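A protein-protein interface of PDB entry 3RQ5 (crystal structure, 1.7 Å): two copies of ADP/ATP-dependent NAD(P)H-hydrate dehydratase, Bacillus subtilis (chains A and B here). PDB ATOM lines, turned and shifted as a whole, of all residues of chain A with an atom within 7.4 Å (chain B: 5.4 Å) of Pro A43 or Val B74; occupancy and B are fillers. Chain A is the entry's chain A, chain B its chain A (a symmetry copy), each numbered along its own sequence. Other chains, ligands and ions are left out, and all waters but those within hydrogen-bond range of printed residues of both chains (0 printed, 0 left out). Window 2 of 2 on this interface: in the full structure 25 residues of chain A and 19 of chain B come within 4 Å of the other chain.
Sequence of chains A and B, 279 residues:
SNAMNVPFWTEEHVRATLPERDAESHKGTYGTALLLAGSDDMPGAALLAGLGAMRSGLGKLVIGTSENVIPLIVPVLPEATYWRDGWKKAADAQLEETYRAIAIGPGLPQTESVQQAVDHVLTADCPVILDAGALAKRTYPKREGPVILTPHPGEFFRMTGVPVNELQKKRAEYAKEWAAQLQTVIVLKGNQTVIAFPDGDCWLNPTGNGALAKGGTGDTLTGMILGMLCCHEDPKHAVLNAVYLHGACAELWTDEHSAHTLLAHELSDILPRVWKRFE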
ATOM      1  N   ALA A  37      -5.009 -19.533  21.692  1.00  0.00           N
ATOM      2  CA  ALA A  37      -5.864 -19.635  20.535  1.00  0.00           C
ATOM      3  C   ALA A  37      -6.179 -18.275  19.978  1.00  0.00           C
ATOM      4  O   ALA A  37      -6.130 -17.271  20.704  1.00  0.00           O
ATOM      5  CB  ALA A  37      -7.185 -20.287  20.967  1.00  0.00           C
ATOM      6  N   GLY A  38      -6.493 -18.244  18.697  1.00  0.00           N
ATOM      7  CA  GLY A  38      -7.000 -17.047  18.004  1.00  0.00           C
ATOM      8  C   GLY A  38      -5.876 -16.182  17.486  1.00  0.00           C
ATOM      9  O   GLY A  38      -4.937 -15.859  18.207  1.00  0.00           O
ATOM     10  N   SER A  39      -5.948 -15.862  16.214  1.00  0.00           N
ATOM     11  CA  SER A  39      -4.949 -15.009  15.578  1.00  0.00           C
ATOM     12  C   SER A  39      -5.699 -13.979  14.793  1.00  0.00           C
ATOM     13  O   SER A  39      -6.926 -14.097  14.539  1.00  0.00           O
ATOM     14  CB  SER A  39      -4.011 -15.837  14.712  1.00  0.00           C
ATOM     15  OG  SER A  39      -4.685 -16.449  13.649  1.00  0.00           O
ATOM     16  N   ASP A  40      -4.972 -12.935  14.394  1.00  0.00           N
ATOM     17  CA  ASP A  40      -5.613 -11.829  13.716  1.00  0.00           C
ATOM     18  C   ASP A  40      -6.369 -12.339  12.512  1.00  0.00           C
ATOM     19  O   ASP A  40      -7.449 -11.871  12.191  1.00  0.00           O
ATOM     20  CB  ASP A  40      -4.572 -10.776  13.282  1.00  0.00           C
ATOM     21  CG  ASP A  40      -4.072  -9.917  14.420  1.00  0.00           C
ATOM     22  OD1 ASP A  40      -4.356 -10.176  15.583  1.00  0.00           O
ATOM     23  OD2 ASP A  40      -3.318  -8.959  14.132  1.00  0.00           O
ATOM     24  N   ASP A  41      -5.809 -13.324  11.831  1.00  0.00           N
ATOM     25  CA  ASP A  41      -6.445 -13.830  10.627  1.00  0.00           C
ATOM     26  C   ASP A  41      -7.597 -14.846  10.932  1.00  0.00           C
ATOM     27  O   ASP A  41      -8.525 -15.023  10.142  1.00  0.00           O
ATOM     28  CB  ASP A  41      -5.377 -14.504   9.720  1.00  0.00           C
ATOM     29  CG  ASP A  41      -4.356 -13.520   9.088  1.00  0.00           C
ATOM     30  OD1 ASP A  41      -4.525 -12.285   9.156  1.00  0.00           O
ATOM     31  OD2 ASP A  41      -3.386 -14.024   8.472  1.00  0.00           O
ATOM     32  N   MET A  42      -7.537 -15.515  12.085  1.00  0.00           N
ATOM     33  CA  MET A  42      -8.567 -16.505  12.512  1.00  0.00           C
ATOM     34  C   MET A  42      -8.996 -16.234  13.979  1.00  0.00           C
ATOM     35  O   MET A  42      -8.682 -17.006  14.891  1.00  0.00           O
ATOM     36  CB  MET A  42      -7.978 -17.928  12.412  1.00  0.00           C
ATOM     37  CG  MET A  42      -7.802 -18.394  10.966  1.00  0.00           C
ATOM     38  SD  MET A  42      -6.863 -19.972  10.946  1.00  0.00           S
ATOM     39  CE  MET A  42      -5.193 -19.398  11.257  1.00  0.00           C
ATOM     40  N   PRO A  43      -9.761 -15.152  14.205  1.00  0.00           N
ATOM     41  CA  PRO A  43     -10.006 -14.700  15.567  1.00  0.00           C
ATOM     42  C   PRO A  43     -11.099 -15.507  16.271  1.00  0.00           C
ATOM     43  O   PRO A  43     -11.084 -15.700  17.483  1.00  0.00           O
ATOM     44  CB  PRO A  43     -10.445 -13.249  15.369  1.00  0.00           C
ATOM     45  CG  PRO A  43     -11.012 -13.201  13.969  1.00  0.00           C
ATOM     46  CD  PRO A  43     -10.140 -14.148  13.197  1.00  0.00           C
ATOM     47  N   GLY A  44     -12.088 -15.956  15.497  1.00  0.00           N
ATOM     48  CA  GLY A  44     -13.294 -16.511  16.080  1.00  0.00           C
ATOM     49  C   GLY A  44     -13.074 -17.766  16.886  1.00  0.00           C
ATOM     50  O   GLY A  44     -13.801 -18.044  17.870  1.00  0.00           O
ATOM     51  N   ALA A  45     -12.039 -18.525  16.513  1.00  0.00           N
ATOM     52  CA  ALA A  45     -11.762 -19.766  17.225  1.00  0.00           C
ATOM     53  C   ALA A  45     -11.502 -19.538  18.728  1.00  0.00           C
ATOM     54  O   ALA A  45     -11.849 -20.381  19.560  1.00  0.00           O
ATOM     55  CB  ALA A  45     -10.577 -20.515  16.584  1.00  0.00           C
ATOM     56  N   ALA A  46     -10.910 -18.405  19.071  1.00  0.00           N
ATOM     57  CA  ALA A  46     -10.667 -18.110  20.465  1.00  0.00           C
ATOM     58  C   ALA A  46     -11.952 -17.876  21.259  1.00  0.00           C
ATOM     59  O   ALA A  46     -12.030 -18.236  22.409  1.00  0.00           O
ATOM     60  CB  ALA A  46      -9.687 -16.902  20.611  1.00  0.00           C
ATOM     61  N   LEU A  47     -12.941 -17.206  20.662  1.00  0.00           N
ATOM     62  CA  LEU A  47     -14.192 -16.957  21.326  1.00  0.00           C
ATOM     63  C   LEU A  47     -14.921 -18.311  21.481  1.00  0.00           C
ATOM     64  O   LEU A  47     -15.451 -18.617  22.553  1.00  0.00           O
ATOM     65  CB  LEU A  47     -15.022 -15.945  20.556  1.00  0.00           C
ATOM     66  CG  LEU A  47     -16.424 -15.698  21.113  1.00  0.00           C
ATOM     67  CD1 LEU A  47     -16.419 -15.421  22.662  1.00  0.00           C
ATOM     68  CD2 LEU A  47     -17.086 -14.500  20.350  1.00  0.00           C
ATOM     69  N   LEU A  48     -14.919 -19.120  20.423  1.00  0.00           N
ATOM     70  CA  LEU A  48     -15.614 -20.415  20.453  1.00  0.00           C
ATOM     71  C   LEU A  48     -15.016 -21.338  21.523  1.00  0.00           C
ATOM     72  O   LEU A  48     -15.732 -21.948  22.326  1.00  0.00           O
ATOM     73  CB  LEU A  48     -15.565 -21.088  19.088  1.00  0.00           C
ATOM     74  CG  LEU A  48     -16.459 -20.385  18.047  1.00  0.00           C
ATOM     75  CD1 LEU A  48     -16.157 -20.966  16.707  1.00  0.00           C
ATOM     76  CD2 LEU A  48     -17.975 -20.561  18.418  1.00  0.00           C
ATOM     77  N   THR A  65      -4.340 -14.898  23.643  1.00  0.00           N
ATOM     78  CA  THR A  65      -4.643 -14.669  22.235  1.00  0.00           C
ATOM     79  C   THR A  65      -3.883 -13.422  21.772  1.00  0.00           C
ATOM     80  O   THR A  65      -3.316 -12.667  22.554  1.00  0.00           O
ATOM     81  CB  THR A  65      -6.115 -14.538  22.007  1.00  0.00           C
ATOM     82  OG1 THR A  65      -6.409 -14.539  20.597  1.00  0.00           O
ATOM     83  CG2 THR A  65      -6.663 -13.285  22.645  1.00  0.00           C
ATOM     84  N   ASN A  68      -5.076  -8.041  19.200  1.00  0.00           N
ATOM     85  CA  ASN A  68      -6.224  -7.503  18.473  1.00  0.00           C
ATOM     86  C   ASN A  68      -7.455  -8.391  18.537  1.00  0.00           C
ATOM     87  O   ASN A  68      -8.550  -7.972  18.156  1.00  0.00           O
ATOM     88  CB  ASN A  68      -5.852  -7.230  17.019  1.00  0.00           C
ATOM     89  CG  ASN A  68      -4.829  -6.120  16.879  1.00  0.00           C
ATOM     90  OD1 ASN A  68      -4.730  -5.213  17.724  1.00  0.00           O
ATOM     91  ND2 ASN A  68      -4.016  -6.214  15.831  1.00  0.00           N
ATOM     92  N   VAL A  69      -7.293  -9.607  19.030  1.00  0.00           N
ATOM     93  CA  VAL A  69      -8.419 -10.534  19.201  1.00  0.00           C
ATOM     94  C   VAL A  69      -9.149 -10.331  20.564  1.00  0.00           C
ATOM     95  O   VAL A  69     -10.361 -10.562  20.713  1.00  0.00           O
ATOM     96  CB  VAL A  69      -7.966 -11.971  19.042  1.00  0.00           C
ATOM     97  CG1 VAL A  69      -9.173 -12.974  19.287  1.00  0.00           C
ATOM     98  CG2 VAL A  69      -7.312 -12.162  17.633  1.00  0.00           C
ATOM     99  N   ILE A  70      -8.388  -9.881  21.562  1.00  0.00           N
ATOM    100  CA  ILE A  70      -8.963  -9.642  22.903  1.00  0.00           C
ATOM    101  C   ILE A  70     -10.279  -8.856  22.886  1.00  0.00           C
ATOM    102  O   ILE A  70     -11.274  -9.319  23.453  1.00  0.00           O
ATOM    103  CB  ILE A  70      -7.948  -9.004  23.849  1.00  0.00           C
ATOM    104  CG1 ILE A  70      -6.779  -9.952  24.071  1.00  0.00           C
ATOM    105  CG2 ILE A  70      -8.591  -8.592  25.194  1.00  0.00           C
ATOM    106  CD1 ILE A  70      -5.628  -9.387  24.909  1.00  0.00           C
ATOM    107  N   LEU A  72     -12.509  -8.593  20.793  1.00  0.00           N
ATOM    108  CA  LEU A  72     -13.587  -9.346  20.138  1.00  0.00           C
ATOM    109  C   LEU A  72     -14.223 -10.385  21.040  1.00  0.00           C
ATOM    110  O   LEU A  72     -15.317 -10.876  20.748  1.00  0.00           O
ATOM    111  CB  LEU A  72     -13.057  -9.990  18.849  1.00  0.00           C
ATOM    112  CG  LEU A  72     -12.233  -9.032  17.965  1.00  0.00           C
ATOM    113  CD1 LEU A  72     -11.831  -9.742  16.648  1.00  0.00           C
ATOM    114  CD2 LEU A  72     -12.984  -7.749  17.722  1.00  0.00           C
ATOM    115  N   ILE A  73     -13.522 -10.767  22.103  1.00  0.00           N
ATOM    116  CA  ILE A  73     -14.001 -11.769  23.037  1.00  0.00           C
ATOM    117  C   ILE A  73     -14.749 -11.148  24.193  1.00  0.00           C
ATOM    118  O   ILE A  73     -15.770 -11.658  24.612  1.00  0.00           O
ATOM    119  CB  ILE A  73     -12.804 -12.623  23.580  1.00  0.00           C
ATOM    120  CG1 ILE A  73     -12.119 -13.369  22.428  1.00  0.00           C
ATOM    121  CG2 ILE A  73     -13.250 -13.603  24.647  1.00  0.00           C
ATOM    122  CD1 ILE A  73     -10.767 -13.988  22.819  1.00  0.00           C
ATOM    123  N   VAL A  76     -18.629 -10.759  24.715  1.00  0.00           N
ATOM    124  CA  VAL A  76     -19.364 -12.034  24.705  1.00  0.00           C
ATOM    125  C   VAL A  76     -19.004 -12.907  25.931  1.00  0.00           C
ATOM    126  O   VAL A  76     -19.890 -13.581  26.503  1.00  0.00           O
ATOM    127  CB  VAL A  76     -19.125 -12.809  23.402  1.00  0.00           C
ATOM    128  CG1 VAL A  76     -19.920 -14.075  23.401  1.00  0.00           C
ATOM    129  CG2 VAL A  76     -19.530 -11.918  22.192  1.00  0.00           C
ATOM    130  N   PRO A 106      -6.482 -23.792  18.314  1.00  0.00           N
ATOM    131  CA  PRO A 106      -7.621 -23.259  17.570  1.00  0.00           C
ATOM    132  C   PRO A 106      -7.302 -21.839  17.066  1.00  0.00           C
ATOM    133  O   PRO A 106      -6.879 -20.953  17.813  1.00  0.00           O
ATOM    134  CB  PRO A 106      -8.760 -23.317  18.573  1.00  0.00           C
ATOM    135  CG  PRO A 106      -8.362 -24.433  19.525  1.00  0.00           C
ATOM    136  CD  PRO A 106      -6.878 -24.252  19.644  1.00  0.00           C
ATOM    137  N   GLY A 107      -7.528 -21.632  15.785  1.00  0.00           N
ATOM    138  CA  GLY A 107      -7.222 -20.338  15.170  1.00  0.00           C
ATOM    139  C   GLY A 107      -5.775 -19.929  15.057  1.00  0.00           C
ATOM    140  O   GLY A 107      -5.502 -18.780  14.782  1.00  0.00           O
ATOM    141  N   HIS A 265     -21.307 -21.793  18.344  1.00  0.00           N
ATOM    142  CA  HIS A 265     -21.433 -21.161  19.670  1.00  0.00           C
ATOM    143  C   HIS A 265     -22.693 -21.584  20.389  1.00  0.00           C
ATOM    144  O   HIS A 265     -22.737 -21.585  21.623  1.00  0.00           O
ATOM    145  CB  HIS A 265     -21.297 -19.650  19.607  1.00  0.00           C
ATOM    146  CG  HIS A 265     -22.475 -18.952  19.016  1.00  0.00           C
ATOM    147  ND1 HIS A 265     -22.548 -18.649  17.675  1.00  0.00           N
ATOM    148  CD2 HIS A 265     -23.599 -18.443  19.587  1.00  0.00           C
ATOM    149  CE1 HIS A 265     -23.682 -18.002  17.441  1.00  0.00           C
ATOM    150  NE2 HIS A 265     -24.341 -17.877  18.577  1.00  0.00           N
ATOM    151  N   ILE B  70     -14.109  -6.607   9.780  1.00  0.00           N
ATOM    152  CA  ILE B  70     -13.878  -7.908  10.444  1.00  0.00           C
ATOM    153  C   ILE B  70     -14.216  -7.914  11.939  1.00  0.00           C
ATOM    154  O   ILE B  70     -14.994  -8.763  12.386  1.00  0.00           O
ATOM    155  CB  ILE B  70     -12.465  -8.429  10.192  1.00  0.00           C
ATOM    156  CG1 ILE B  70     -12.265  -8.689   8.707  1.00  0.00           C
ATOM    157  CG2 ILE B  70     -12.160  -9.697  11.023  1.00  0.00           C
ATOM    158  CD1 ILE B  70     -10.849  -9.104   8.300  1.00  0.00           C
ATOM    159  N   PRO B  71     -13.665  -6.987  12.712  1.00  0.00           N
ATOM    160  CA  PRO B  71     -13.922  -7.014  14.147  1.00  0.00           C
ATOM    161  C   PRO B  71     -15.402  -6.815  14.533  1.00  0.00           C
ATOM    162  O   PRO B  71     -15.799  -7.168  15.654  1.00  0.00           O
ATOM    163  CB  PRO B  71     -13.052  -5.905  14.704  1.00  0.00           C
ATOM    164  CG  PRO B  71     -12.738  -5.072  13.576  1.00  0.00           C
ATOM    165  CD  PRO B  71     -12.718  -5.925  12.371  1.00  0.00           C
ATOM    166  N   LEU B  72     -16.200  -6.284  13.622  1.00  0.00           N
ATOM    167  CA  LEU B  72     -17.635  -6.080  13.859  1.00  0.00           C
ATOM    168  C   LEU B  72     -18.455  -7.341  13.673  1.00  0.00           C
ATOM    169  O   LEU B  72     -19.603  -7.408  14.120  1.00  0.00           O
ATOM    170  CB  LEU B  72     -18.152  -4.952  12.956  1.00  0.00           C
ATOM    171  CG  LEU B  72     -17.257  -3.695  12.951  1.00  0.00           C
ATOM    172  CD1 LEU B  72     -17.913  -2.582  12.095  1.00  0.00           C
ATOM    173  CD2 LEU B  72     -16.963  -3.243  14.358  1.00  0.00           C
ATOM    174  N   ILE B  73     -17.899  -8.320  12.964  1.00  0.00           N
ATOM    175  CA  ILE B  73     -18.581  -9.571  12.690  1.00  0.00           C
ATOM    176  C   ILE B  73     -18.266 -10.621  13.728  1.00  0.00           C
ATOM    177  O   ILE B  73     -19.142 -11.350  14.153  1.00  0.00           O
ATOM    178  CB  ILE B  73     -18.192 -10.102  11.267  1.00  0.00           C
ATOM    179  CG1 ILE B  73     -18.631  -9.102  10.190  1.00  0.00           C
ATOM    180  CG2 ILE B  73     -18.793 -11.466  10.991  1.00  0.00           C
ATOM    181  CD1 ILE B  73     -18.032  -9.394   8.804  1.00  0.00           C
ATOM    182  N   VAL B  74     -17.006 -10.700  14.114  1.00  0.00           N
ATOM    183  CA  VAL B  74     -16.515 -11.803  14.951  1.00  0.00           C
ATOM    184  C   VAL B  74     -17.346 -12.107  16.203  1.00  0.00           C
ATOM    185  O   VAL B  74     -17.694 -13.246  16.452  1.00  0.00           O
ATOM    186  CB  VAL B  74     -15.018 -11.598  15.272  1.00  0.00           C
ATOM    187  CG1 VAL B  74     -14.530 -12.711  16.242  1.00  0.00           C
ATOM    188  CG2 VAL B  74     -14.199 -11.560  13.994  1.00  0.00           C
ATOM    189  N   PRO B  75     -17.693 -11.089  17.009  1.00  0.00           N
ATOM    190  CA  PRO B  75     -18.418 -11.430  18.256  1.00  0.00           C
ATOM    191  C   PRO B  75     -19.784 -12.020  18.015  1.00  0.00           C
ATOM    192  O   PRO B  75     -20.289 -12.766  18.874  1.00  0.00           O
ATOM    193  CB  PRO B  75     -18.573 -10.087  18.960  1.00  0.00           C
ATOM    194  CG  PRO B  75     -17.704  -9.127  18.219  1.00  0.00           C
ATOM    195  CD  PRO B  75     -17.395  -9.659  16.890  1.00  0.00           C
ATOM    196  N   VAL B  76     -20.376 -11.722  16.861  1.00  0.00           N
ATOM    197  CA  VAL B  76     -21.725 -12.211  16.532  1.00  0.00           C
ATOM    198  C   VAL B  76     -21.671 -13.545  15.749  1.00  0.00           C
ATOM    199  O   VAL B  76     -22.519 -14.439  15.973  1.00  0.00           O
ATOM    200  CB  VAL B  76     -22.527 -11.160  15.751  1.00  0.00           C
ATOM    201  CG1 VAL B  76     -23.906 -11.665  15.472  1.00  0.00           C
ATOM    202  CG2 VAL B  76     -22.593  -9.844  16.580  1.00  0.00           C
ATOM    203  N   LEU B  77     -20.623 -13.692  14.936  1.00  0.00           N
ATOM    204  CA  LEU B  77     -20.481 -14.828  14.036  1.00  0.00           C
ATOM    205  C   LEU B  77     -19.038 -15.350  14.122  1.00  0.00           C
ATOM    206  O   LEU B  77     -18.243 -15.220  13.160  1.00  0.00           O
ATOM    207  CB  LEU B  77     -20.858 -14.400  12.613  1.00  0.00           C
ATOM    208  CG  LEU B  77     -20.998 -15.550  11.602  1.00  0.00           C
ATOM    209  CD1 LEU B  77     -22.115 -16.579  11.921  1.00  0.00           C
ATOM    210  CD2 LEU B  77     -21.144 -14.946  10.158  1.00  0.00           C
ATOM    211  N   PRO B  78     -18.668 -15.918  15.284  1.00  0.00           N
ATOM    212  CA  PRO B  78     -17.250 -16.327  15.441  1.00  0.00           C
ATOM    213  C   PRO B  78     -16.906 -17.573  14.616  1.00  0.00           C
ATOM    214  O   PRO B  78     -15.753 -17.972  14.552  1.00  0.00           O
ATOM    215  CB  PRO B  78     -17.124 -16.556  16.938  1.00  0.00           C
ATOM    216  CG  PRO B  78     -18.563 -16.966  17.354  1.00  0.00           C
ATOM    217  CD  PRO B  78     -19.422 -16.043  16.541  1.00  0.00           C
ATOM    218  N   TYR B  82     -11.919 -15.368   7.489  1.00  0.00           N
ATOM    219  CA  TYR B  82     -11.773 -14.094   6.729  1.00  0.00           C
ATOM    220  C   TYR B  82     -10.700 -14.150   5.639  1.00  0.00           C
ATOM    221  O   TYR B  82      -9.697 -14.834   5.777  1.00  0.00           O
ATOM    222  CB  TYR B  82     -11.496 -12.900   7.686  1.00  0.00           C
ATOM    223  CG  TYR B  82     -12.588 -12.770   8.689  1.00  0.00           C
ATOM    224  CD1 TYR B  82     -13.760 -12.128   8.369  1.00  0.00           C
ATOM    225  CD2 TYR B  82     -12.509 -13.417   9.909  1.00  0.00           C
ATOM    226  CE1 TYR B  82     -14.795 -12.086   9.231  1.00  0.00           C
ATOM    227  CE2 TYR B  82     -13.570 -13.427  10.777  1.00  0.00           C
ATOM    228  CZ  TYR B  82     -14.706 -12.738  10.444  1.00  0.00           C
ATOM    229  OH  TYR B  82     -15.807 -12.716  11.245  1.00  0.00           O
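Positions printed for both chains: 70, 72, 73 and 76.
Of the 10 pairs that touch across the chains among the printed residues, none has its exchanged pair printed and touching as well.
Among the printed residues, merely in contact across the chains: Gly A44 with Pro B78 (3.2 Å), Val A76 with Pro B75 (3.5 Å), Leu A72 with Pro B71 (3.5 Å), Pro A43 with Val B74 (3.6 Å), Leu A48 with Pro B78 (3.7 Å), Leu A72 with Pro B75 (3.8 Å), Leu A47 with Pro B75 (3.9 Å), Leu A72 with Val B74 (3.9 Å), Leu A47 with Pro B78 (3.98 Å) and Gly A44 with Val B74 (3.999 Å).
Pro A43 touches just one residue of chain B: Val B74.
Printed residues of chain A within 4 Å of Val B74: Pro A43 (3.6 Å), Gly A44 (3.999 Å) and Leu A72 (3.9 Å).
Of the printed residues of chain A, Pro B71 touches Leu A72 (3.5 Å).
Of the printed residues of chain B, Leu A48 touches Pro B78 (3.7 Å).
Printed residues of chain B within 4 Å of Gly A44: Val B74 (3.999 Å) and Pro B78 (3.2 Å).
Asn A68 touches none of the printed residues of chain B.
Ile A70 touches none of the printed residues of chain B.
The nearest residue of chain B that does not touch Pro A43 is Tyr B82 (4.1 Å).
Of the 10 printed residues of chain B, 4 touch a printed residue of chain A.
Printed residues of chain B that touch a printed residue of chain A: Pro B71, Val B74, Pro B75 and Pro B78.
Of the 22 printed residues of chain A, 6 touch a printed residue of chain B.
Among the printed residues, 10 pairs touch across the chains.
Among the printed residues, no Asp or Glu carboxylate lies within 4 Å of a Lys or Arg side-chain nitrogen of the other chain.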
